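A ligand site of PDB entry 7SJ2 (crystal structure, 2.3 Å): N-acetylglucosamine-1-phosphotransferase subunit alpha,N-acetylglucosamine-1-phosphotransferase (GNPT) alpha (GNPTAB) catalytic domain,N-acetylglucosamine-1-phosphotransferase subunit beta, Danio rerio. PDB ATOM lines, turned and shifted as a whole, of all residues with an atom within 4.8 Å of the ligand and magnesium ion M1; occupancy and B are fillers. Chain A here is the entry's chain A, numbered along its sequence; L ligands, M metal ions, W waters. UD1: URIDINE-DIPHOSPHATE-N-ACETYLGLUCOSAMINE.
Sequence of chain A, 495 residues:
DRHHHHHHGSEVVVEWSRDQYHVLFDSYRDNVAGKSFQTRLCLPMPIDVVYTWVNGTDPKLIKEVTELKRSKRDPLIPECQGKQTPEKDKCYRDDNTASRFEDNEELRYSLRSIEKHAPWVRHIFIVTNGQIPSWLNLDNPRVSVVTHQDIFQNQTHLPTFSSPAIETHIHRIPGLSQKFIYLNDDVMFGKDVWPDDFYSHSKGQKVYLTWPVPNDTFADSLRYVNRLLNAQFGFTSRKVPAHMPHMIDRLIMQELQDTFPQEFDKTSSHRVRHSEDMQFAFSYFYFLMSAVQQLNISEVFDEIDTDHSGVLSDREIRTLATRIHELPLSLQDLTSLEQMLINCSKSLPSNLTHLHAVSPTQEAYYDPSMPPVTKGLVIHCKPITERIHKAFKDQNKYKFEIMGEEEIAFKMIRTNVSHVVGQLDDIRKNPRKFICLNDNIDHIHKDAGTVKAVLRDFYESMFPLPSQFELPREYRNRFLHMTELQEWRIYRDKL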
ATOM      1  N   THR A  52     -21.769  22.398  17.324  1.00  0.00           N
ATOM      2  CA  THR A  52     -21.840  23.840  17.481  1.00  0.00           C
ATOM      3  C   THR A  52     -21.193  24.488  16.265  1.00  0.00           C
ATOM      4  O   THR A  52     -20.245  23.960  15.684  1.00  0.00           O
ATOM      5  CB  THR A  52     -21.142  24.327  18.762  1.00  0.00           C
ATOM      6  OG1 THR A  52     -19.832  23.750  18.848  1.00  0.00           O
ATOM      7  CG2 THR A  52     -21.955  23.947  19.990  1.00  0.00           C
ATOM      8  N   TRP A  53     -21.740  25.637  15.872  1.00  0.00           N
ATOM      9  CA  TRP A  53     -21.256  26.319  14.687  1.00  0.00           C
ATOM     10  C   TRP A  53     -21.464  27.816  14.844  1.00  0.00           C
ATOM     11  O   TRP A  53     -22.495  28.262  15.358  1.00  0.00           O
ATOM     12  CB  TRP A  53     -21.967  25.826  13.433  1.00  0.00           C
ATOM     13  CG  TRP A  53     -21.441  26.425  12.156  1.00  0.00           C
ATOM     14  CD1 TRP A  53     -20.266  26.116  11.534  1.00  0.00           C
ATOM     15  CD2 TRP A  53     -22.073  27.435  11.362  1.00  0.00           C
ATOM     16  NE1 TRP A  53     -20.133  26.866  10.396  1.00  0.00           N
ATOM     17  CE2 TRP A  53     -21.235  27.674  10.262  1.00  0.00           C
ATOM     18  CE3 TRP A  53     -23.267  28.146  11.465  1.00  0.00           C
ATOM     19  CZ2 TRP A  53     -21.542  28.606   9.280  1.00  0.00           C
ATOM     20  CZ3 TRP A  53     -23.576  29.065  10.479  1.00  0.00           C
ATOM     21  CH2 TRP A  53     -22.723  29.288   9.401  1.00  0.00           C
ATOM     22  N   VAL A  54     -20.494  28.583  14.371  1.00  0.00           N
ATOM     23  CA  VAL A  54     -20.559  30.033  14.362  1.00  0.00           C
ATOM     24  C   VAL A  54     -19.967  30.510  13.043  1.00  0.00           C
ATOM     25  O   VAL A  54     -19.086  29.862  12.469  1.00  0.00           O
ATOM     26  CB  VAL A  54     -19.825  30.648  15.566  1.00  0.00           C
ATOM     27  CG1 VAL A  54     -18.327  30.287  15.530  1.00  0.00           C
ATOM     28  CG2 VAL A  54     -20.029  32.161  15.606  1.00  0.00           C
ATOM     29  N   SER A  99      -9.805  33.557  14.558  1.00  0.00           N
ATOM     30  CA  SER A  99      -9.686  32.107  14.572  1.00  0.00           C
ATOM     31  C   SER A  99     -10.734  31.432  15.446  1.00  0.00           C
ATOM     32  O   SER A  99     -11.017  30.251  15.251  1.00  0.00           O
ATOM     33  CB  SER A  99      -8.286  31.700  15.050  1.00  0.00           C
ATOM     34  OG  SER A  99      -7.302  31.997  14.076  1.00  0.00           O
ATOM     35  N   ARG A 100     -11.316  32.160  16.400  1.00  0.00           N
ATOM     36  CA  ARG A 100     -12.357  31.573  17.243  1.00  0.00           C
ATOM     37  C   ARG A 100     -13.638  31.324  16.467  1.00  0.00           C
ATOM     38  O   ARG A 100     -14.403  30.405  16.802  1.00  0.00           O
ATOM     39  CB  ARG A 100     -12.658  32.485  18.428  1.00  0.00           C
ATOM     40  CG  ARG A 100     -11.555  32.587  19.448  1.00  0.00           C
ATOM     41  CD  ARG A 100     -11.627  31.480  20.484  1.00  0.00           C
ATOM     42  NE  ARG A 100     -10.723  31.751  21.599  1.00  0.00           N
ATOM     43  CZ  ARG A 100      -9.617  31.085  21.861  1.00  0.00           C
ATOM     44  NH1 ARG A 100      -9.224  30.058  21.117  1.00  0.00           N
ATOM     45  NH2 ARG A 100      -8.867  31.447  22.903  1.00  0.00           N
ATOM     46  N   PHE A 101     -13.904  32.115  15.416  1.00  0.00           N
ATOM     47  CA  PHE A 101     -15.240  32.160  14.830  1.00  0.00           C
ATOM     48  C   PHE A 101     -15.272  31.890  13.336  1.00  0.00           C
ATOM     49  O   PHE A 101     -16.372  31.812  12.770  1.00  0.00           O
ATOM     50  CB  PHE A 101     -15.876  33.521  15.108  1.00  0.00           C
ATOM     51  CG  PHE A 101     -15.703  33.994  16.522  1.00  0.00           C
ATOM     52  CD1 PHE A 101     -16.390  33.398  17.563  1.00  0.00           C
ATOM     53  CD2 PHE A 101     -14.841  35.040  16.811  1.00  0.00           C
ATOM     54  CE1 PHE A 101     -16.227  33.834  18.869  1.00  0.00           C
ATOM     55  CE2 PHE A 101     -14.680  35.487  18.108  1.00  0.00           C
ATOM     56  CZ  PHE A 101     -15.375  34.880  19.138  1.00  0.00           C
ATOM     57  N   VAL A 127     -26.165  23.584  16.897  1.00  0.00           N
ATOM     58  CA  VAL A 127     -26.427  24.615  17.896  1.00  0.00           C
ATOM     59  C   VAL A 127     -25.727  25.897  17.475  1.00  0.00           C
ATOM     60  O   VAL A 127     -24.513  25.909  17.254  1.00  0.00           O
ATOM     61  CB  VAL A 127     -25.944  24.155  19.288  1.00  0.00           C
ATOM     62  CG1 VAL A 127     -26.113  25.270  20.313  1.00  0.00           C
ATOM     63  CG2 VAL A 127     -26.707  22.918  19.732  1.00  0.00           C
ATOM     64  N   THR A 160     -23.749  35.122  23.604  1.00  0.00           N
ATOM     65  CA  THR A 160     -22.477  34.585  24.074  1.00  0.00           C
ATOM     66  C   THR A 160     -21.533  34.365  22.903  1.00  0.00           C
ATOM     67  O   THR A 160     -21.958  34.223  21.747  1.00  0.00           O
ATOM     68  CB  THR A 160     -22.668  33.273  24.837  1.00  0.00           C
ATOM     69  OG1 THR A 160     -21.442  32.928  25.491  1.00  0.00           O
ATOM     70  CG2 THR A 160     -23.069  32.141  23.887  1.00  0.00           C
ATOM     71  N   PHE A 161     -20.243  34.344  23.232  1.00  0.00           N
ATOM     72  CA  PHE A 161     -19.202  34.074  22.255  1.00  0.00           C
ATOM     73  C   PHE A 161     -18.167  33.120  22.849  1.00  0.00           C
ATOM     74  O   PHE A 161     -16.976  33.196  22.512  1.00  0.00           O
ATOM     75  CB  PHE A 161     -18.551  35.375  21.788  1.00  0.00           C
ATOM     76  CG  PHE A 161     -19.554  36.413  21.360  1.00  0.00           C
ATOM     77  CD1 PHE A 161     -20.143  36.361  20.111  1.00  0.00           C
ATOM     78  CD2 PHE A 161     -19.949  37.414  22.229  1.00  0.00           C
ATOM     79  CE1 PHE A 161     -21.077  37.292  19.718  1.00  0.00           C
ATOM     80  CE2 PHE A 161     -20.887  38.351  21.843  1.00  0.00           C
ATOM     81  CZ  PHE A 161     -21.448  38.289  20.591  1.00  0.00           C
ATOM     82  N   SER A 162     -18.616  32.234  23.736  1.00  0.00           N
ATOM     83  CA  SER A 162     -17.732  31.339  24.479  1.00  0.00           C
ATOM     84  C   SER A 162     -18.192  29.909  24.249  1.00  0.00           C
ATOM     85  O   SER A 162     -19.306  29.542  24.643  1.00  0.00           O
ATOM     86  CB  SER A 162     -17.755  31.676  25.967  1.00  0.00           C
ATOM     87  OG  SER A 162     -17.220  30.634  26.759  1.00  0.00           O
ATOM     88  N   SER A 163     -17.351  29.097  23.620  1.00  0.00           N
ATOM     89  CA  SER A 163     -17.721  27.701  23.415  1.00  0.00           C
ATOM     90  C   SER A 163     -17.891  26.949  24.738  1.00  0.00           C
ATOM     91  O   SER A 163     -18.851  26.173  24.854  1.00  0.00           O
ATOM     92  CB  SER A 163     -16.714  26.999  22.494  1.00  0.00           C
ATOM     93  OG  SER A 163     -15.378  27.000  22.964  1.00  0.00           O
ATOM     94  N   PRO A 164     -17.070  27.172  25.771  1.00  0.00           N
ATOM     95  CA  PRO A 164     -17.330  26.454  27.038  1.00  0.00           C
ATOM     96  C   PRO A 164     -18.692  26.765  27.632  1.00  0.00           C
ATOM     97  O   PRO A 164     -19.355  25.861  28.165  1.00  0.00           O
ATOM     98  CB  PRO A 164     -16.190  26.936  27.947  1.00  0.00           C
ATOM     99  CG  PRO A 164     -15.110  27.378  27.021  1.00  0.00           C
ATOM    100  CD  PRO A 164     -15.825  27.954  25.826  1.00  0.00           C
ATOM    101  N   ILE A 166     -21.485  27.710  25.972  1.00  0.00           N
ATOM    102  CA  ILE A 166     -22.462  27.025  25.139  1.00  0.00           C
ATOM    103  C   ILE A 166     -22.485  25.540  25.480  1.00  0.00           C
ATOM    104  O   ILE A 166     -23.547  24.921  25.585  1.00  0.00           O
ATOM    105  CB  ILE A 166     -22.133  27.249  23.648  1.00  0.00           C
ATOM    106  CG1 ILE A 166     -22.264  28.732  23.302  1.00  0.00           C
ATOM    107  CG2 ILE A 166     -23.056  26.426  22.780  1.00  0.00           C
ATOM    108  CD1 ILE A 166     -21.623  29.100  21.979  1.00  0.00           C
ATOM    109  N   GLU A 167     -21.300  24.953  25.661  1.00  0.00           N
ATOM    110  CA  GLU A 167     -21.192  23.520  25.858  1.00  0.00           C
ATOM    111  C   GLU A 167     -21.767  23.066  27.197  1.00  0.00           C
ATOM    112  O   GLU A 167     -22.087  21.879  27.338  1.00  0.00           O
ATOM    113  CB  GLU A 167     -19.729  23.095  25.696  1.00  0.00           C
ATOM    114  CG  GLU A 167     -19.259  23.200  24.251  1.00  0.00           C
ATOM    115  CD  GLU A 167     -17.748  23.213  24.080  1.00  0.00           C
ATOM    116  OE1 GLU A 167     -17.012  23.454  25.059  1.00  0.00           O
ATOM    117  OE2 GLU A 167     -17.288  22.972  22.940  1.00  0.00           O
ATOM    118  N   TYR A 182     -20.983  14.656  20.523  1.00  0.00           N
ATOM    119  CA  TYR A 182     -20.769  16.074  20.286  1.00  0.00           C
ATOM    120  C   TYR A 182     -19.520  16.263  19.426  1.00  0.00           C
ATOM    121  O   TYR A 182     -18.435  15.820  19.799  1.00  0.00           O
ATOM    122  CB  TYR A 182     -20.600  16.817  21.603  1.00  0.00           C
ATOM    123  CG  TYR A 182     -20.150  18.248  21.427  1.00  0.00           C
ATOM    124  CD1 TYR A 182     -20.840  19.105  20.572  1.00  0.00           C
ATOM    125  CD2 TYR A 182     -19.057  18.739  22.106  1.00  0.00           C
ATOM    126  CE1 TYR A 182     -20.438  20.405  20.408  1.00  0.00           C
ATOM    127  CE2 TYR A 182     -18.648  20.061  21.943  1.00  0.00           C
ATOM    128  CZ  TYR A 182     -19.347  20.883  21.083  1.00  0.00           C
ATOM    129  OH  TYR A 182     -18.960  22.190  20.906  1.00  0.00           O
ATOM    130  N   ASN A 184     -17.298  19.376  17.625  1.00  0.00           N
ATOM    131  CA  ASN A 184     -16.961  20.700  17.134  1.00  0.00           C
ATOM    132  C   ASN A 184     -17.080  20.686  15.608  1.00  0.00           C
ATOM    133  O   ASN A 184     -16.917  19.653  14.965  1.00  0.00           O
ATOM    134  CB  ASN A 184     -15.533  21.083  17.541  1.00  0.00           C
ATOM    135  CG  ASN A 184     -15.381  21.390  19.031  1.00  0.00           C
ATOM    136  OD1 ASN A 184     -14.428  22.049  19.429  1.00  0.00           O
ATOM    137  ND2 ASN A 184     -16.310  20.911  19.862  1.00  0.00           N
ATOM    138  N   ASP A 185     -17.349  21.860  15.026  1.00  0.00           N
ATOM    139  CA  ASP A 185     -17.437  21.919  13.573  1.00  0.00           C
ATOM    140  C   ASP A 185     -16.138  21.494  12.909  1.00  0.00           C
ATOM    141  O   ASP A 185     -16.167  20.928  11.801  1.00  0.00           O
ATOM    142  CB  ASP A 185     -17.830  23.333  13.111  1.00  0.00           C
ATOM    143  CG  ASP A 185     -16.760  24.371  13.390  1.00  0.00           C
ATOM    144  OD1 ASP A 185     -16.055  24.264  14.410  1.00  0.00           O
ATOM    145  OD2 ASP A 185     -16.635  25.314  12.577  1.00  0.00           O
ATOM    146  N   ASP A 186     -14.988  21.738  13.549  1.00  0.00           N
ATOM    147  CA  ASP A 186     -13.694  21.433  12.938  1.00  0.00           C
ATOM    148  C   ASP A 186     -13.235  20.001  13.220  1.00  0.00           C
ATOM    149  O   ASP A 186     -12.087  19.668  12.943  1.00  0.00           O
ATOM    150  CB  ASP A 186     -12.639  22.439  13.399  1.00  0.00           C
ATOM    151  CG  ASP A 186     -12.447  22.465  14.899  1.00  0.00           C
ATOM    152  OD1 ASP A 186     -12.729  21.449  15.562  1.00  0.00           O
ATOM    153  OD2 ASP A 186     -12.010  23.520  15.407  1.00  0.00           O
ATOM    154  N   VAL A 187     -14.127  19.161  13.732  1.00  0.00           N
ATOM    155  CA  VAL A 187     -13.858  17.751  13.965  1.00  0.00           C
ATOM    156  C   VAL A 187     -14.685  16.959  12.965  1.00  0.00           C
ATOM    157  O   VAL A 187     -15.827  17.316  12.662  1.00  0.00           O
ATOM    158  CB  VAL A 187     -14.201  17.372  15.408  1.00  0.00           C
ATOM    159  CG1 VAL A 187     -14.147  15.883  15.593  1.00  0.00           C
ATOM    160  CG2 VAL A 187     -13.254  18.087  16.388  1.00  0.00           C
ATOM    161  N   ALA A 242      -8.536  13.627  24.180  1.00  0.00           N
ATOM    162  CA  ALA A 242      -8.215  13.989  22.812  1.00  0.00           C
ATOM    163  C   ALA A 242      -9.216  14.996  22.250  1.00  0.00           C
ATOM    164  O   ALA A 242     -10.360  15.071  22.688  1.00  0.00           O
ATOM    165  CB  ALA A 242      -8.201  12.744  21.925  1.00  0.00           C
ATOM    166  N   HIS A 243      -8.755  15.785  21.281  1.00  0.00           N
ATOM    167  CA  HIS A 243      -9.613  16.690  20.515  1.00  0.00           C
ATOM    168  C   HIS A 243     -10.323  15.854  19.466  1.00  0.00           C
ATOM    169  O   HIS A 243      -9.783  15.576  18.392  1.00  0.00           O
ATOM    170  CB  HIS A 243      -8.805  17.803  19.855  1.00  0.00           C
ATOM    171  CG  HIS A 243      -8.082  18.680  20.832  1.00  0.00           C
ATOM    172  ND1 HIS A 243      -8.706  19.677  21.549  1.00  0.00           N
ATOM    173  CD2 HIS A 243      -6.776  18.713  21.196  1.00  0.00           C
ATOM    174  CE1 HIS A 243      -7.818  20.273  22.318  1.00  0.00           C
ATOM    175  NE2 HIS A 243      -6.641  19.713  22.129  1.00  0.00           N
ATOM    176  N   MET A 244     -11.544  15.442  19.774  1.00  0.00           N
ATOM    177  CA  MET A 244     -12.241  14.471  18.942  1.00  0.00           C
ATOM    178  C   MET A 244     -13.742  14.575  19.192  1.00  0.00           C
ATOM    179  O   MET A 244     -14.165  15.334  20.068  1.00  0.00           O
ATOM    180  CB  MET A 244     -11.740  13.069  19.281  1.00  0.00           C
ATOM    181  CG  MET A 244     -12.096  12.652  20.707  1.00  0.00           C
ATOM    182  SD  MET A 244     -11.647  10.955  21.072  1.00  0.00           S
ATOM    183  CE  MET A 244     -12.810  10.022  20.065  1.00  0.00           C
ATOM    184  N   HIS A 246     -16.999  13.552  21.050  1.00  0.00           N
ATOM    185  CA  HIS A 246     -17.156  13.090  22.418  1.00  0.00           C
ATOM    186  C   HIS A 246     -18.558  12.541  22.634  1.00  0.00           C
ATOM    187  O   HIS A 246     -19.542  13.270  22.465  1.00  0.00           O
ATOM    188  CB  HIS A 246     -16.910  14.218  23.422  1.00  0.00           C
ATOM    189  CG  HIS A 246     -15.514  14.758  23.402  1.00  0.00           C
ATOM    190  ND1 HIS A 246     -14.406  13.970  23.597  1.00  0.00           N
ATOM    191  CD2 HIS A 246     -15.062  16.032  23.235  1.00  0.00           C
ATOM    192  CE1 HIS A 246     -13.319  14.722  23.536  1.00  0.00           C
ATOM    193  NE2 HIS A 246     -13.691  15.979  23.318  1.00  0.00           N
ATOM    194  N   ARG A 273     -14.346  33.157  26.453  1.00  0.00           N
ATOM    195  CA  ARG A 273     -13.494  32.176  27.120  1.00  0.00           C
ATOM    196  C   ARG A 273     -12.865  32.760  28.376  1.00  0.00           C
ATOM    197  O   ARG A 273     -12.403  33.896  28.382  1.00  0.00           O
ATOM    198  CB  ARG A 273     -12.397  31.714  26.172  1.00  0.00           C
ATOM    199  CG  ARG A 273     -12.506  30.287  25.743  1.00  0.00           C
ATOM    200  CD  ARG A 273     -11.539  30.004  24.628  1.00  0.00           C
ATOM    201  NE  ARG A 273     -12.229  29.352  23.514  1.00  0.00           N
ATOM    202  CZ  ARG A 273     -11.823  28.249  22.905  1.00  0.00           C
ATOM    203  NH1 ARG A 273     -10.672  27.675  23.216  1.00  0.00           N
ATOM    204  NH2 ARG A 273     -12.585  27.723  21.959  1.00  0.00           N
ATOM    205  N   GLN A 279     -13.985  22.994  31.722  1.00  0.00           N
ATOM    206  CA  GLN A 279     -13.700  22.464  30.392  1.00  0.00           C
ATOM    207  C   GLN A 279     -14.561  21.246  30.109  1.00  0.00           C
ATOM    208  O   GLN A 279     -14.634  20.312  30.916  1.00  0.00           O
ATOM    209  CB  GLN A 279     -12.216  22.110  30.283  1.00  0.00           C
ATOM    210  CG  GLN A 279     -11.631  22.225  28.885  1.00  0.00           C
ATOM    211  CD  GLN A 279     -12.041  21.082  27.956  1.00  0.00           C
ATOM    212  OE1 GLN A 279     -12.082  19.916  28.354  1.00  0.00           O
ATOM    213  NE2 GLN A 279     -12.347  21.422  26.706  1.00  0.00           N
ATOM    214  N   CYS A 436      -9.196  16.394  13.674  1.00  0.00           N
ATOM    215  CA  CYS A 436      -9.470  17.758  14.100  1.00  0.00           C
ATOM    216  C   CYS A 436      -8.456  18.687  13.452  1.00  0.00           C
ATOM    217  O   CYS A 436      -7.255  18.576  13.718  1.00  0.00           O
ATOM    218  CB  CYS A 436      -9.400  17.880  15.631  1.00  0.00           C
ATOM    219  SG  CYS A 436      -9.677  19.559  16.232  1.00  0.00           S
ATOM    220  N   ASN A 438      -7.599  22.325  13.603  1.00  0.00           N
ATOM    221  CA  ASN A 438      -7.894  23.442  14.490  1.00  0.00           C
ATOM    222  C   ASN A 438      -7.356  24.748  13.918  1.00  0.00           C
ATOM    223  O   ASN A 438      -6.228  24.813  13.433  1.00  0.00           O
ATOM    224  CB  ASN A 438      -7.291  23.191  15.872  1.00  0.00           C
ATOM    225  CG  ASN A 438      -8.323  23.288  16.965  1.00  0.00           C
ATOM    226  OD1 ASN A 438      -9.508  23.030  16.744  1.00  0.00           O
ATOM    227  ND2 ASN A 438      -7.879  23.660  18.163  1.00  0.00           N
HETATM  228  C1' UD1 L   1     -11.418  22.937  22.226  1.00  0.00           C
HETATM  229  C2' UD1 L   1     -12.540  21.921  22.488  1.00  0.00           C
HETATM  230  C3' UD1 L   1     -13.832  22.713  22.664  1.00  0.00           C
HETATM  231  C4' UD1 L   1     -13.655  23.579  23.904  1.00  0.00           C
HETATM  232  C5' UD1 L   1     -12.534  24.573  23.588  1.00  0.00           C
HETATM  233  C6' UD1 L   1     -12.204  25.394  24.816  1.00  0.00           C
HETATM  234  C7' UD1 L   1     -12.469  19.755  21.353  1.00  0.00           C
HETATM  235  C8' UD1 L   1     -12.634  19.029  20.053  1.00  0.00           C
HETATM  236  N2' UD1 L   1     -12.649  21.071  21.319  1.00  0.00           N
HETATM  237  O1' UD1 L   1     -11.948  23.588  21.078  1.00  0.00           O
HETATM  238  O3' UD1 L   1     -14.830  21.750  22.968  1.00  0.00           O
HETATM  239  O4' UD1 L   1     -14.830  24.373  24.018  1.00  0.00           O
HETATM  240  O5' UD1 L   1     -11.343  23.825  23.325  1.00  0.00           O
HETATM  241  O6' UD1 L   1     -12.364  24.666  26.020  1.00  0.00           O
HETATM  242  O7' UD1 L   1     -12.195  19.157  22.399  1.00  0.00           O
HETATM  243  N1  UD1 L   1     -18.351  28.014  18.693  1.00  0.00           N
HETATM  244  C2  UD1 L   1     -19.628  28.518  18.589  1.00  0.00           C
HETATM  245  N3  UD1 L   1     -19.755  29.853  18.896  1.00  0.00           N
HETATM  246  C4  UD1 L   1     -18.742  30.714  19.283  1.00  0.00           C
HETATM  247  C5  UD1 L   1     -17.440  30.116  19.368  1.00  0.00           C
HETATM  248  C6  UD1 L   1     -17.290  28.810  19.079  1.00  0.00           C
HETATM  249  O2  UD1 L   1     -20.586  27.840  18.263  1.00  0.00           O
HETATM  250  O4  UD1 L   1     -19.004  31.899  19.521  1.00  0.00           O
HETATM  251  C1B UD1 L   1     -18.140  26.592  18.398  1.00  0.00           C
HETATM  252  C2B UD1 L   1     -17.123  26.429  17.280  1.00  0.00           C
HETATM  253  O2' UD1 L   1     -17.926  26.309  16.106  1.00  0.00           O
HETATM  254  C3B UD1 L   1     -16.600  25.021  17.579  1.00  0.00           C
HETATM  255  C4B UD1 L   1     -16.671  24.942  19.100  1.00  0.00           C
HETATM  256  O4B UD1 L   1     -17.491  26.047  19.510  1.00  0.00           O
HETATM  257  O3B UD1 L   1     -17.577  24.127  17.052  1.00  0.00           O
HETATM  258  C5B UD1 L   1     -15.304  25.131  19.732  1.00  0.00           C
HETATM  259  O5B UD1 L   1     -14.638  26.268  19.154  1.00  0.00           O
HETATM  260  PA  UD1 L   1     -13.110  26.201  18.755  1.00  0.00           P
HETATM  261  O1A UD1 L   1     -12.653  27.506  18.252  1.00  0.00           O
HETATM  262  O2A UD1 L   1     -12.942  25.027  17.812  1.00  0.00           O
HETATM  263  O3A UD1 L   1     -12.384  25.821  20.122  1.00  0.00           O
HETATM  264  PB  UD1 L   1     -11.199  24.864  20.575  1.00  0.00           P
HETATM  265  O1B UD1 L   1     -10.323  25.592  21.513  1.00  0.00           O
HETATM  266  O2B UD1 L   1     -10.461  24.474  19.281  1.00  0.00           O
HETATM  267 MG    MG M   1     -11.164  23.950  17.349  1.00  0.00          MG
HETATM  268 MG    MG M   2     -13.154  27.279  14.182  1.00  0.00          MG
HETATM  269  O   HOH W   1     -14.003  19.787  25.226  1.00  0.00           O
HETATM  270  O   HOH W   2     -12.121  22.146  17.990  1.00  0.00           O
HETATM  271  O   HOH W   3     -10.282  28.868  18.972  1.00  0.00           O
HETATM  272  O   HOH W   4     -14.178  25.898  15.497  1.00  0.00           O
HETATM  273  O   HOH W   5     -22.316  31.016  18.368  1.00  0.00           O
HETATM  274  O   HOH W   6     -10.393  25.704  16.460  1.00  0.00           O
HETATM  275  O   HOH W   7      -7.839  23.512  21.515  1.00  0.00           O
HETATM  276  O   HOH W   8     -23.121  27.517  19.011  1.00  0.00           O
HETATM  277  O   HOH W   9     -21.389  33.468  19.242  1.00  0.00           O
HETATM  278  O   HOH W  10     -11.835  25.879  28.484  1.00  0.00           O
HETATM  279  O   HOH W  11     -14.075  29.266  19.787  1.00  0.00           O
HETATM  280  O   HOH W  12     -17.331  27.898  13.601  1.00  0.00           O
HETATM  281  O   HOH W  13     -15.210  23.589  27.296  1.00  0.00           O
HETATM  282  O   HOH W  14     -12.127  28.022  15.867  1.00  0.00           O
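An oxygen (O4') of the ligand is in hydrogen-bond range of the side-chain carboxylate (OE1) of Glu 167 (2.6 Å). The guanidinium group of Arg 273 lies within salt-bridge range of an oxygen (O1B) of the ligand (2.7 Å). N2' of the ligand is in hydrogen-bond range of OD1 of Asn 184, at 2.8 Å. OG of Ser 163 lies within hydrogen-bond range of O4' of the ligand (2.9 Å). O of Thr 52 is in hydrogen-bond range of O3B of the ligand. OG1 of Thr 52 lies within hydrogen-bond range of O3B of the ligand, at 2.9 Å. An oxygen (O3B) of the ligand sits at hydrogen-bond distance from the backbone NH (N) of Asp 185 (3.0 Å). The side-chain carboxylate (OD1) of Asp 185 lies within hydrogen-bond range of an oxygen (O3B) of the ligand. The side-chain amide nitrogen of Gln 279 is in hydrogen-bond range of an oxygen (O6') of the ligand (3.3 Å). The backbone NH of Trp 53 lies within hydrogen-bond range of an oxygen (O2) of the ligand (3.4 Å).
The side-chain sulfur (SG) of Cys 436 lies close to the side-chain amide oxygen (OD1) of Asn 438. The side-chain sulfur of Cys 436 sits at hydrogen-bond distance from the side-chain carboxylate of Asp 186. OE2 of Glu 167 sits at hydrogen-bond distance from OH of Tyr 182. NH2 of Arg 273 is in hydrogen-bond range of OG of Ser 163, at 3.1 Å. ND2 of Asn 184 lies within hydrogen-bond range of OH of Tyr 182 (3.1 Å). The side-chain hydroxyl (OG1) of Thr 52 sits at hydrogen-bond distance from the side-chain hydroxyl (OH) of Tyr 182, at 2.7 Å. The backbone NH (N) of Trp 53 lies within hydrogen-bond range of the backbone carbonyl oxygen (O) of Val 127 (3.1 Å). The backbone carbonyl oxygen of His 246 sits at hydrogen-bond distance from the backbone NH of Tyr 182 (2.8 Å).
Val 54 touches the ligand. Arg 100 touches the ligand (O to O1A, 3.7 Å). Phe 101 touches the ligand. Phe 161 touches the ligand. Pro 164 touches the ligand (CG to O6', 3.99 Å). CD1 of Ile 166 touches N3 of the ligand, 3.7 Å away. Val 187 touches the ligand (CG2 to C8', 3.8 Å). His 243 touches the ligand (ND1 to O7', 3.6 Å). Met 244 touches the ligand (N to C8', 3.8 Å). NE2 of His 246 touches O7' of the ligand, at 3.6 Å. Hydrophobic or aromatic side chains that line the ligand: Val 54, Phe 101, Pro 164, Ile 166 and Val 187. The nearest printed residue that does not touch the ligand is Tyr 182 (4.01 Å).
Of the 27 residues printed, 2 come within 4 Å of magnesium ion M1.
Magnesium ion M1 is bound by the side-chain amide oxygen (OD1) of Asn 438 (2.0 Å). Magnesium ion M1 is bound by water W6, 2.1 Å away. Magnesium ion M1 is bound by an oxygen (O2B) of the ligand, 2.1 Å away. Magnesium ion M1 is bound by O2A of the ligand (2.1 Å). Magnesium ion M1 is bound by water W2. OD2 of Asp 186 binds magnesium ion M1 (2.2 Å). Magnesium ion M1 has six donor atoms within binding distance.
Water W11 lies within hydrogen-bond range of O1A of the ligand (2.7 Å), NH2 of Arg 273 (3.1 Å) and O of Arg 100 (3.2 Å). Water W3 bridges NH1 of Arg 100 (2.7 Å) and O1A of the ligand (2.8 Å). Water W9 lies within hydrogen-bond range of O of Thr 160 (2.7 Å) and O4 of the ligand (2.9 Å). Water W12 lies within hydrogen-bond range of the side-chain carboxylate (OD2) of Asp 185 (2.9 Å), the backbone carbonyl oxygen (O) of Val 54 (2.9 Å) and an oxygen (O2') of the ligand (3.0 Å). Water W1 lies within hydrogen-bond range of the side-chain amide nitrogen of Gln 279 (2.8 Å) and an oxygen (O3') of the ligand (3.1 Å). Water W13 lies within hydrogen-bond range of the side-chain carboxylate (OE1) of Glu 167 and an oxygen (O6') of the ligand.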
